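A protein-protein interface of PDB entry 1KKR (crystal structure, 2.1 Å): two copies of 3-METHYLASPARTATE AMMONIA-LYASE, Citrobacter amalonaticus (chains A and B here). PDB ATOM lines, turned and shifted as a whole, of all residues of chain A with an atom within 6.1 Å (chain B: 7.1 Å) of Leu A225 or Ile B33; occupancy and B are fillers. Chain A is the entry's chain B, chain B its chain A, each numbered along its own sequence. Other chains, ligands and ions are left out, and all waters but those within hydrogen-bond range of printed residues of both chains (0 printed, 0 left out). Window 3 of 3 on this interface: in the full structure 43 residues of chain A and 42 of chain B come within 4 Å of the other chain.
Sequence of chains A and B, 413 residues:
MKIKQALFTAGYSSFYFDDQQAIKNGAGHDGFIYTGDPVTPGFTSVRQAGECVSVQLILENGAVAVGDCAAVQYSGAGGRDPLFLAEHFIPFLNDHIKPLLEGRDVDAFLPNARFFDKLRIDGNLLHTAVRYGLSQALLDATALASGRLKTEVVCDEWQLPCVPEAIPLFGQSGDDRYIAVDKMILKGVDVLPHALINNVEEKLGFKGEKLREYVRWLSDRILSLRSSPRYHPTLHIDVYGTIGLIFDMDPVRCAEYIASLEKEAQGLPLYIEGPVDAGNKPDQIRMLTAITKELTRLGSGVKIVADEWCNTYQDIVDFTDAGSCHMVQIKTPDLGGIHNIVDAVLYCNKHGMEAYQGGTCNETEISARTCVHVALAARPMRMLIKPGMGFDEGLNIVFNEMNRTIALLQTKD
OD1 of Asp B30 lies within salt-bridge range of NH1 of Arg A221 (3.1 Å). The backbone NH of Phe B32 sits at hydrogen-bond distance from the side-chain carboxylate of Asp A182 (3.0 Å).
The backbone carbonyl oxygen of Phe B32 sits at hydrogen-bond distance from the guanidinium group of Arg B47 (3.1 Å). The guanidinium group of Arg A221 lies within salt-bridge range of the side-chain carboxylate of Asp A182 (2.8 Å).
Among the printed residues, merely in contact across the chains: Leu A186 with Ile B33, Asp A182 with Gly B31, Leu A225 with Ile B33 and Asp A182 with Asp B30.
Of the printed residues of chain B, Leu A225 touches Ile B33 (3.9 Å). Of chain A, only Leu A186 (3.5 Å) and Leu A225 (3.9 Å) come within 4 Å of Ile B33. Printed residues of chain A within 4 Å of Asp B30: Asp A182 and Arg A221. Printed residues of chain B within 4 Å of Arg A221: Asp B30. Of the printed residues of chain B, Leu A186 touches Ile B33. Printed residues of chain A within 4 Å of Gly B31: Asp A182 (3.7 Å). Printed residues of chain A within 4 Å of Phe B32: Asp A182. Gly B28 touches none of the printed residues of chain A. Ser A227 touches none of the printed residues of chain B. The nearest printed residue of chain A that does not touch Asp B30 is Leu A225 (5.5 Å).
Printed residues of chain A that touch a printed residue of chain B: Asp A182, Leu A186, Arg A221 and Leu A225. Hydrophobic or aromatic side chains of chain A that line the printed part of chain B: Leu A186 and Leu A225. Among the printed residues, Asp or Glu carboxylates within 4 Å of a Lys or Arg side-chain nitrogen of the other chain: Arg A221 with Asp B30.
No position is printed for both chains. Of the 6 pairs that touch across the chains among the printed residues, none has its exchanged pair printed and touching as well.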
ATOM      1  N   ASP A 182      23.402  10.204 -14.730  1.00  0.00           N
ATOM      2  CA  ASP A 182      22.722  10.398 -16.004  1.00  0.00           C
ATOM      3  C   ASP A 182      21.903   9.148 -16.443  1.00  0.00           C
ATOM      4  O   ASP A 182      20.797   9.249 -17.037  1.00  0.00           O
ATOM      5  CB  ASP A 182      23.695  10.745 -17.114  1.00  0.00           C
ATOM      6  CG  ASP A 182      24.360  12.096 -16.923  1.00  0.00           C
ATOM      7  OD1 ASP A 182      23.859  12.955 -16.177  1.00  0.00           O
ATOM      8  OD2 ASP A 182      25.373  12.379 -17.548  1.00  0.00           O
ATOM      9  N   ILE A 185      18.629   9.081 -14.570  1.00  0.00           N
ATOM     10  CA  ILE A 185      17.641  10.035 -15.030  1.00  0.00           C
ATOM     11  C   ILE A 185      17.094   9.467 -16.327  1.00  0.00           C
ATOM     12  O   ILE A 185      15.928   9.557 -16.589  1.00  0.00           O
ATOM     13  CB  ILE A 185      18.244  11.378 -15.304  1.00  0.00           C
ATOM     14  CG1 ILE A 185      18.512  12.148 -13.988  1.00  0.00           C
ATOM     15  CG2 ILE A 185      17.323  12.132 -16.088  1.00  0.00           C
ATOM     16  CD1 ILE A 185      19.684  12.998 -14.066  1.00  0.00           C
ATOM     17  N   LEU A 186      17.947   8.915 -17.170  1.00  0.00           N
ATOM     18  CA  LEU A 186      17.452   8.474 -18.462  1.00  0.00           C
ATOM     19  C   LEU A 186      16.508   7.307 -18.281  1.00  0.00           C
ATOM     20  O   LEU A 186      15.636   7.109 -19.098  1.00  0.00           O
ATOM     21  CB  LEU A 186      18.580   8.084 -19.384  1.00  0.00           C
ATOM     22  CG  LEU A 186      19.423   9.109 -20.119  1.00  0.00           C
ATOM     23  CD1 LEU A 186      20.613   8.405 -20.776  1.00  0.00           C
ATOM     24  CD2 LEU A 186      18.611   9.833 -21.178  1.00  0.00           C
ATOM     25  N   ASP A 220      20.433  19.950  -9.930  1.00  0.00           N
ATOM     26  CA  ASP A 220      20.491  20.629 -11.188  1.00  0.00           C
ATOM     27  C   ASP A 220      20.484  19.598 -12.336  1.00  0.00           C
ATOM     28  O   ASP A 220      19.809  19.814 -13.340  1.00  0.00           O
ATOM     29  CB  ASP A 220      21.795  21.427 -11.319  1.00  0.00           C
ATOM     30  CG  ASP A 220      21.787  22.766 -10.559  1.00  0.00           C
ATOM     31  OD1 ASP A 220      20.705  23.331 -10.311  1.00  0.00           O
ATOM     32  OD2 ASP A 220      22.854  23.351 -10.235  1.00  0.00           O
ATOM     33  N   ARG A 221      21.240  18.497 -12.205  1.00  0.00           N
ATOM     34  CA  ARG A 221      21.353  17.546 -13.323  1.00  0.00           C
ATOM     35  C   ARG A 221      19.969  16.995 -13.638  1.00  0.00           C
ATOM     36  O   ARG A 221      19.575  16.901 -14.775  1.00  0.00           O
ATOM     37  CB  ARG A 221      22.306  16.389 -13.005  1.00  0.00           C
ATOM     38  CG  ARG A 221      22.769  15.636 -14.233  1.00  0.00           C
ATOM     39  CD  ARG A 221      23.556  16.509 -15.208  1.00  0.00           C
ATOM     40  NE  ARG A 221      24.177  15.690 -16.245  1.00  0.00           N
ATOM     41  CZ  ARG A 221      24.840  16.143 -17.324  1.00  0.00           C
ATOM     42  NH1 ARG A 221      25.026  17.461 -17.577  1.00  0.00           N
ATOM     43  NH2 ARG A 221      25.335  15.243 -18.167  1.00  0.00           N
ATOM     44  N   ILE A 222      19.273  16.581 -12.586  1.00  0.00           N
ATOM     45  CA  ILE A 222      17.970  16.032 -12.699  1.00  0.00           C
ATOM     46  C   ILE A 222      17.060  17.027 -13.392  1.00  0.00           C
ATOM     47  O   ILE A 222      16.407  16.663 -14.366  1.00  0.00           O
ATOM     48  CB  ILE A 222      17.419  15.664 -11.327  1.00  0.00           C
ATOM     49  CG1 ILE A 222      18.233  14.492 -10.778  1.00  0.00           C
ATOM     50  CG2 ILE A 222      15.983  15.272 -11.492  1.00  0.00           C
ATOM     51  CD1 ILE A 222      17.982  13.961  -9.317  1.00  0.00           C
ATOM     52  N   LEU A 223      17.015  18.262 -12.883  1.00  0.00           N
ATOM     53  CA  LEU A 223      16.129  19.304 -13.410  1.00  0.00           C
ATOM     54  C   LEU A 223      16.533  19.702 -14.811  1.00  0.00           C
ATOM     55  O   LEU A 223      15.691  20.070 -15.597  1.00  0.00           O
ATOM     56  CB  LEU A 223      16.059  20.576 -12.541  1.00  0.00           C
ATOM     57  CG  LEU A 223      15.718  20.448 -11.049  1.00  0.00           C
ATOM     58  CD1 LEU A 223      15.829  21.815 -10.359  1.00  0.00           C
ATOM     59  CD2 LEU A 223      14.407  19.817 -10.735  1.00  0.00           C
ATOM     60  N   SER A 224      17.804  19.566 -15.139  1.00  0.00           N
ATOM     61  CA  SER A 224      18.219  19.857 -16.488  1.00  0.00           C
ATOM     62  C   SER A 224      17.943  18.699 -17.458  1.00  0.00           C
ATOM     63  O   SER A 224      17.349  18.888 -18.501  1.00  0.00           O
ATOM     64  CB  SER A 224      19.684  20.192 -16.462  1.00  0.00           C
ATOM     65  OG  SER A 224      20.165  20.205 -17.755  1.00  0.00           O
ATOM     66  N   LEU A 225      18.300  17.482 -17.093  1.00  0.00           N
ATOM     67  CA  LEU A 225      18.150  16.361 -18.018  1.00  0.00           C
ATOM     68  C   LEU A 225      16.773  15.758 -18.237  1.00  0.00           C
ATOM     69  O   LEU A 225      16.534  15.067 -19.242  1.00  0.00           O
ATOM     70  CB  LEU A 225      18.981  15.194 -17.517  1.00  0.00           C
ATOM     71  CG  LEU A 225      20.294  15.040 -18.242  1.00  0.00           C
ATOM     72  CD1 LEU A 225      20.061  14.726 -19.751  1.00  0.00           C
ATOM     73  CD2 LEU A 225      21.004  16.375 -18.041  1.00  0.00           C
ATOM     74  N   ARG A 226      15.911  15.913 -17.263  1.00  0.00           N
ATOM     75  CA  ARG A 226      14.655  15.204 -17.288  1.00  0.00           C
ATOM     76  C   ARG A 226      13.793  15.690 -18.404  1.00  0.00           C
ATOM     77  O   ARG A 226      13.844  16.846 -18.760  1.00  0.00           O
ATOM     78  CB  ARG A 226      13.921  15.421 -15.992  1.00  0.00           C
ATOM     79  CG  ARG A 226      13.394  16.792 -15.779  1.00  0.00           C
ATOM     80  CD  ARG A 226      12.811  16.931 -14.385  1.00  0.00           C
ATOM     81  NE  ARG A 226      12.310  18.273 -14.152  1.00  0.00           N
ATOM     82  CZ  ARG A 226      11.702  18.684 -13.043  1.00  0.00           C
ATOM     83  NH1 ARG A 226      11.471  17.869 -12.043  1.00  0.00           N
ATOM     84  NH2 ARG A 226      11.289  19.928 -12.944  1.00  0.00           N
ATOM     85  N   SER A 227      12.912  14.856 -18.904  1.00  0.00           N
ATOM     86  CA  SER A 227      12.077  15.354 -20.000  1.00  0.00           C
ATOM     87  C   SER A 227      10.867  16.178 -19.562  1.00  0.00           C
ATOM     88  O   SER A 227      10.414  16.989 -20.342  1.00  0.00           O
ATOM     89  CB  SER A 227      11.612  14.232 -20.914  1.00  0.00           C
ATOM     90  OG  SER A 227      10.857  13.297 -20.176  1.00  0.00           O
ATOM     91  N   GLY B  28      29.338  15.000 -29.861  1.00  0.00           N
ATOM     92  CA  GLY B  28      29.976  15.254 -28.593  1.00  0.00           C
ATOM     93  C   GLY B  28      29.219  14.688 -27.400  1.00  0.00           C
ATOM     94  O   GLY B  28      28.083  14.192 -27.495  1.00  0.00           O
ATOM     95  N   HIS B  29      29.882  14.761 -26.256  1.00  0.00           N
ATOM     96  CA  HIS B  29      29.280  14.291 -25.036  1.00  0.00           C
ATOM     97  C   HIS B  29      29.205  15.324 -23.928  1.00  0.00           C
ATOM     98  O   HIS B  29      29.883  16.350 -23.950  1.00  0.00           O
ATOM     99  CB  HIS B  29      29.890  12.981 -24.572  1.00  0.00           C
ATOM    100  CG  HIS B  29      31.370  12.984 -24.346  1.00  0.00           C
ATOM    101  ND1 HIS B  29      31.918  13.006 -23.080  1.00  0.00           N
ATOM    102  CD2 HIS B  29      32.406  12.795 -25.198  1.00  0.00           C
ATOM    103  CE1 HIS B  29      33.233  12.909 -23.168  1.00  0.00           C
ATOM    104  NE2 HIS B  29      33.557  12.781 -24.442  1.00  0.00           N
ATOM    105  N   ASP B  30      28.309  15.041 -22.991  1.00  0.00           N
ATOM    106  CA  ASP B  30      28.131  15.822 -21.782  1.00  0.00           C
ATOM    107  C   ASP B  30      27.804  14.724 -20.776  1.00  0.00           C
ATOM    108  O   ASP B  30      26.685  14.227 -20.766  1.00  0.00           O
ATOM    109  CB  ASP B  30      26.977  16.800 -21.973  1.00  0.00           C
ATOM    110  CG  ASP B  30      26.573  17.535 -20.686  1.00  0.00           C
ATOM    111  OD1 ASP B  30      27.290  17.464 -19.652  1.00  0.00           O
ATOM    112  OD2 ASP B  30      25.524  18.231 -20.653  1.00  0.00           O
ATOM    113  N   GLY B  31      28.792  14.309 -19.983  1.00  0.00           N
ATOM    114  CA  GLY B  31      28.660  13.191 -19.042  1.00  0.00           C
ATOM    115  C   GLY B  31      28.384  11.908 -19.837  1.00  0.00           C
ATOM    116  O   GLY B  31      29.092  11.607 -20.756  1.00  0.00           O
ATOM    117  N   PHE B  32      27.276  11.229 -19.574  1.00  0.00           N
ATOM    118  CA  PHE B  32      26.931   9.995 -20.265  1.00  0.00           C
ATOM    119  C   PHE B  32      26.107  10.250 -21.472  1.00  0.00           C
ATOM    120  O   PHE B  32      25.880   9.358 -22.264  1.00  0.00           O
ATOM    121  CB  PHE B  32      26.106   9.147 -19.350  1.00  0.00           C
ATOM    122  CG  PHE B  32      25.991   7.717 -19.774  1.00  0.00           C
ATOM    123  CD1 PHE B  32      27.118   6.883 -19.845  1.00  0.00           C
ATOM    124  CD2 PHE B  32      24.745   7.206 -20.106  1.00  0.00           C
ATOM    125  CE1 PHE B  32      26.986   5.531 -20.215  1.00  0.00           C
ATOM    126  CE2 PHE B  32      24.593   5.891 -20.488  1.00  0.00           C
ATOM    127  CZ  PHE B  32      25.711   5.038 -20.551  1.00  0.00           C
ATOM    128  N   ILE B  33      25.633  11.466 -21.607  1.00  0.00           N
ATOM    129  CA  ILE B  33      24.760  11.843 -22.703  1.00  0.00           C
ATOM    130  C   ILE B  33      25.551  12.287 -23.951  1.00  0.00           C
ATOM    131  O   ILE B  33      26.652  12.827 -23.813  1.00  0.00           O
ATOM    132  CB  ILE B  33      23.894  13.037 -22.208  1.00  0.00           C
ATOM    133  CG1 ILE B  33      23.047  12.600 -21.031  1.00  0.00           C
ATOM    134  CG2 ILE B  33      22.996  13.618 -23.311  1.00  0.00           C
ATOM    135  CD1 ILE B  33      22.221  11.429 -21.355  1.00  0.00           C
ATOM    136  N   TYR B  34      24.996  12.031 -25.146  1.00  0.00           N
ATOM    137  CA  TYR B  34      25.555  12.514 -26.398  1.00  0.00           C
ATOM    138  C   TYR B  34      24.775  13.748 -26.770  1.00  0.00           C
ATOM    139  O   TYR B  34      23.555  13.799 -26.542  1.00  0.00           O
ATOM    140  CB  TYR B  34      25.407  11.491 -27.492  1.00  0.00           C
ATOM    141  CG  TYR B  34      26.499  10.499 -27.453  1.00  0.00           C
ATOM    142  CD1 TYR B  34      27.754  10.832 -27.888  1.00  0.00           C
ATOM    143  CD2 TYR B  34      26.300   9.252 -26.925  1.00  0.00           C
ATOM    144  CE1 TYR B  34      28.796   9.930 -27.829  1.00  0.00           C
ATOM    145  CE2 TYR B  34      27.332   8.334 -26.870  1.00  0.00           C
ATOM    146  CZ  TYR B  34      28.570   8.684 -27.328  1.00  0.00           C
ATOM    147  OH  TYR B  34      29.601   7.790 -27.287  1.00  0.00           O
ATOM    148  N   THR B  35      25.495  14.754 -27.265  1.00  0.00           N
ATOM    149  CA  THR B  35      24.922  16.020 -27.739  1.00  0.00           C
ATOM    150  C   THR B  35      24.637  16.073 -29.249  1.00  0.00           C
ATOM    151  O   THR B  35      25.097  15.239 -30.036  1.00  0.00           O
ATOM    152  CB  THR B  35      25.904  17.183 -27.418  1.00  0.00           C
ATOM    153  OG1 THR B  35      27.160  16.957 -28.088  1.00  0.00           O
ATOM    154  CG2 THR B  35      26.304  17.211 -25.921  1.00  0.00           C
ATOM    155  N   SER B  45      16.941  11.197 -28.751  1.00  0.00           N
ATOM    156  CA  SER B  45      18.252  11.706 -28.425  1.00  0.00           C
ATOM    157  C   SER B  45      19.298  10.820 -29.050  1.00  0.00           C
ATOM    158  O   SER B  45      18.992   9.760 -29.544  1.00  0.00           O
ATOM    159  CB  SER B  45      18.390  11.687 -26.942  1.00  0.00           C
ATOM    160  OG  SER B  45      17.174  12.146 -26.437  1.00  0.00           O
ATOM    161  N   VAL B  46      20.537  11.262 -29.061  1.00  0.00           N
ATOM    162  CA  VAL B  46      21.560  10.446 -29.649  1.00  0.00           C
ATOM    163  C   VAL B  46      21.655   9.124 -28.838  1.00  0.00           C
ATOM    164  O   VAL B  46      21.836   8.045 -29.402  1.00  0.00           O
ATOM    165  CB  VAL B  46      22.873  11.244 -29.802  1.00  0.00           C
ATOM    166  CG1 VAL B  46      23.976  10.359 -30.288  1.00  0.00           C
ATOM    167  CG2 VAL B  46      22.691  12.311 -30.873  1.00  0.00           C
ATOM    168  N   ARG B  47      21.486   9.233 -27.526  1.00  0.00           N
ATOM    169  CA  ARG B  47      21.497   8.086 -26.624  1.00  0.00           C
ATOM    170  C   ARG B  47      20.217   8.107 -25.829  1.00  0.00           C
ATOM    171  O   ARG B  47      19.867   9.144 -25.272  1.00  0.00           O
ATOM    172  CB  ARG B  47      22.664   8.177 -25.683  1.00  0.00           C
ATOM    173  CG  ARG B  47      22.578   7.214 -24.550  1.00  0.00           C
ATOM    174  CD  ARG B  47      23.865   7.078 -23.820  1.00  0.00           C
ATOM    175  NE  ARG B  47      24.734   6.113 -24.518  1.00  0.00           N
ATOM    176  CZ  ARG B  47      26.012   5.873 -24.218  1.00  0.00           C
ATOM    177  NH1 ARG B  47      26.728   4.964 -24.876  1.00  0.00           N
ATOM    178  NH2 ARG B  47      26.595   6.523 -23.248  1.00  0.00           N
ATOM    179  N   GLN B  48      19.527   6.964 -25.805  1.00  0.00           N
ATOM    180  CA  GLN B  48      18.254   6.773 -25.083  1.00  0.00           C
ATOM    181  C   GLN B  48      18.276   5.455 -24.313  1.00  0.00           C
ATOM    182  O   GLN B  48      19.013   4.541 -24.669  1.00  0.00           O
ATOM    183  CB  GLN B  48      17.067   6.567 -26.068  1.00  0.00           C
ATOM    184  CG  GLN B  48      16.822   7.628 -27.105  1.00  0.00           C
ATOM    185  CD  GLN B  48      15.549   7.426 -27.929  1.00  0.00           C
ATOM    186  OE1 GLN B  48      15.513   7.857 -29.077  1.00  0.00           O
ATOM    187  NE2 GLN B  48      14.523   6.760 -27.365  1.00  0.00           N
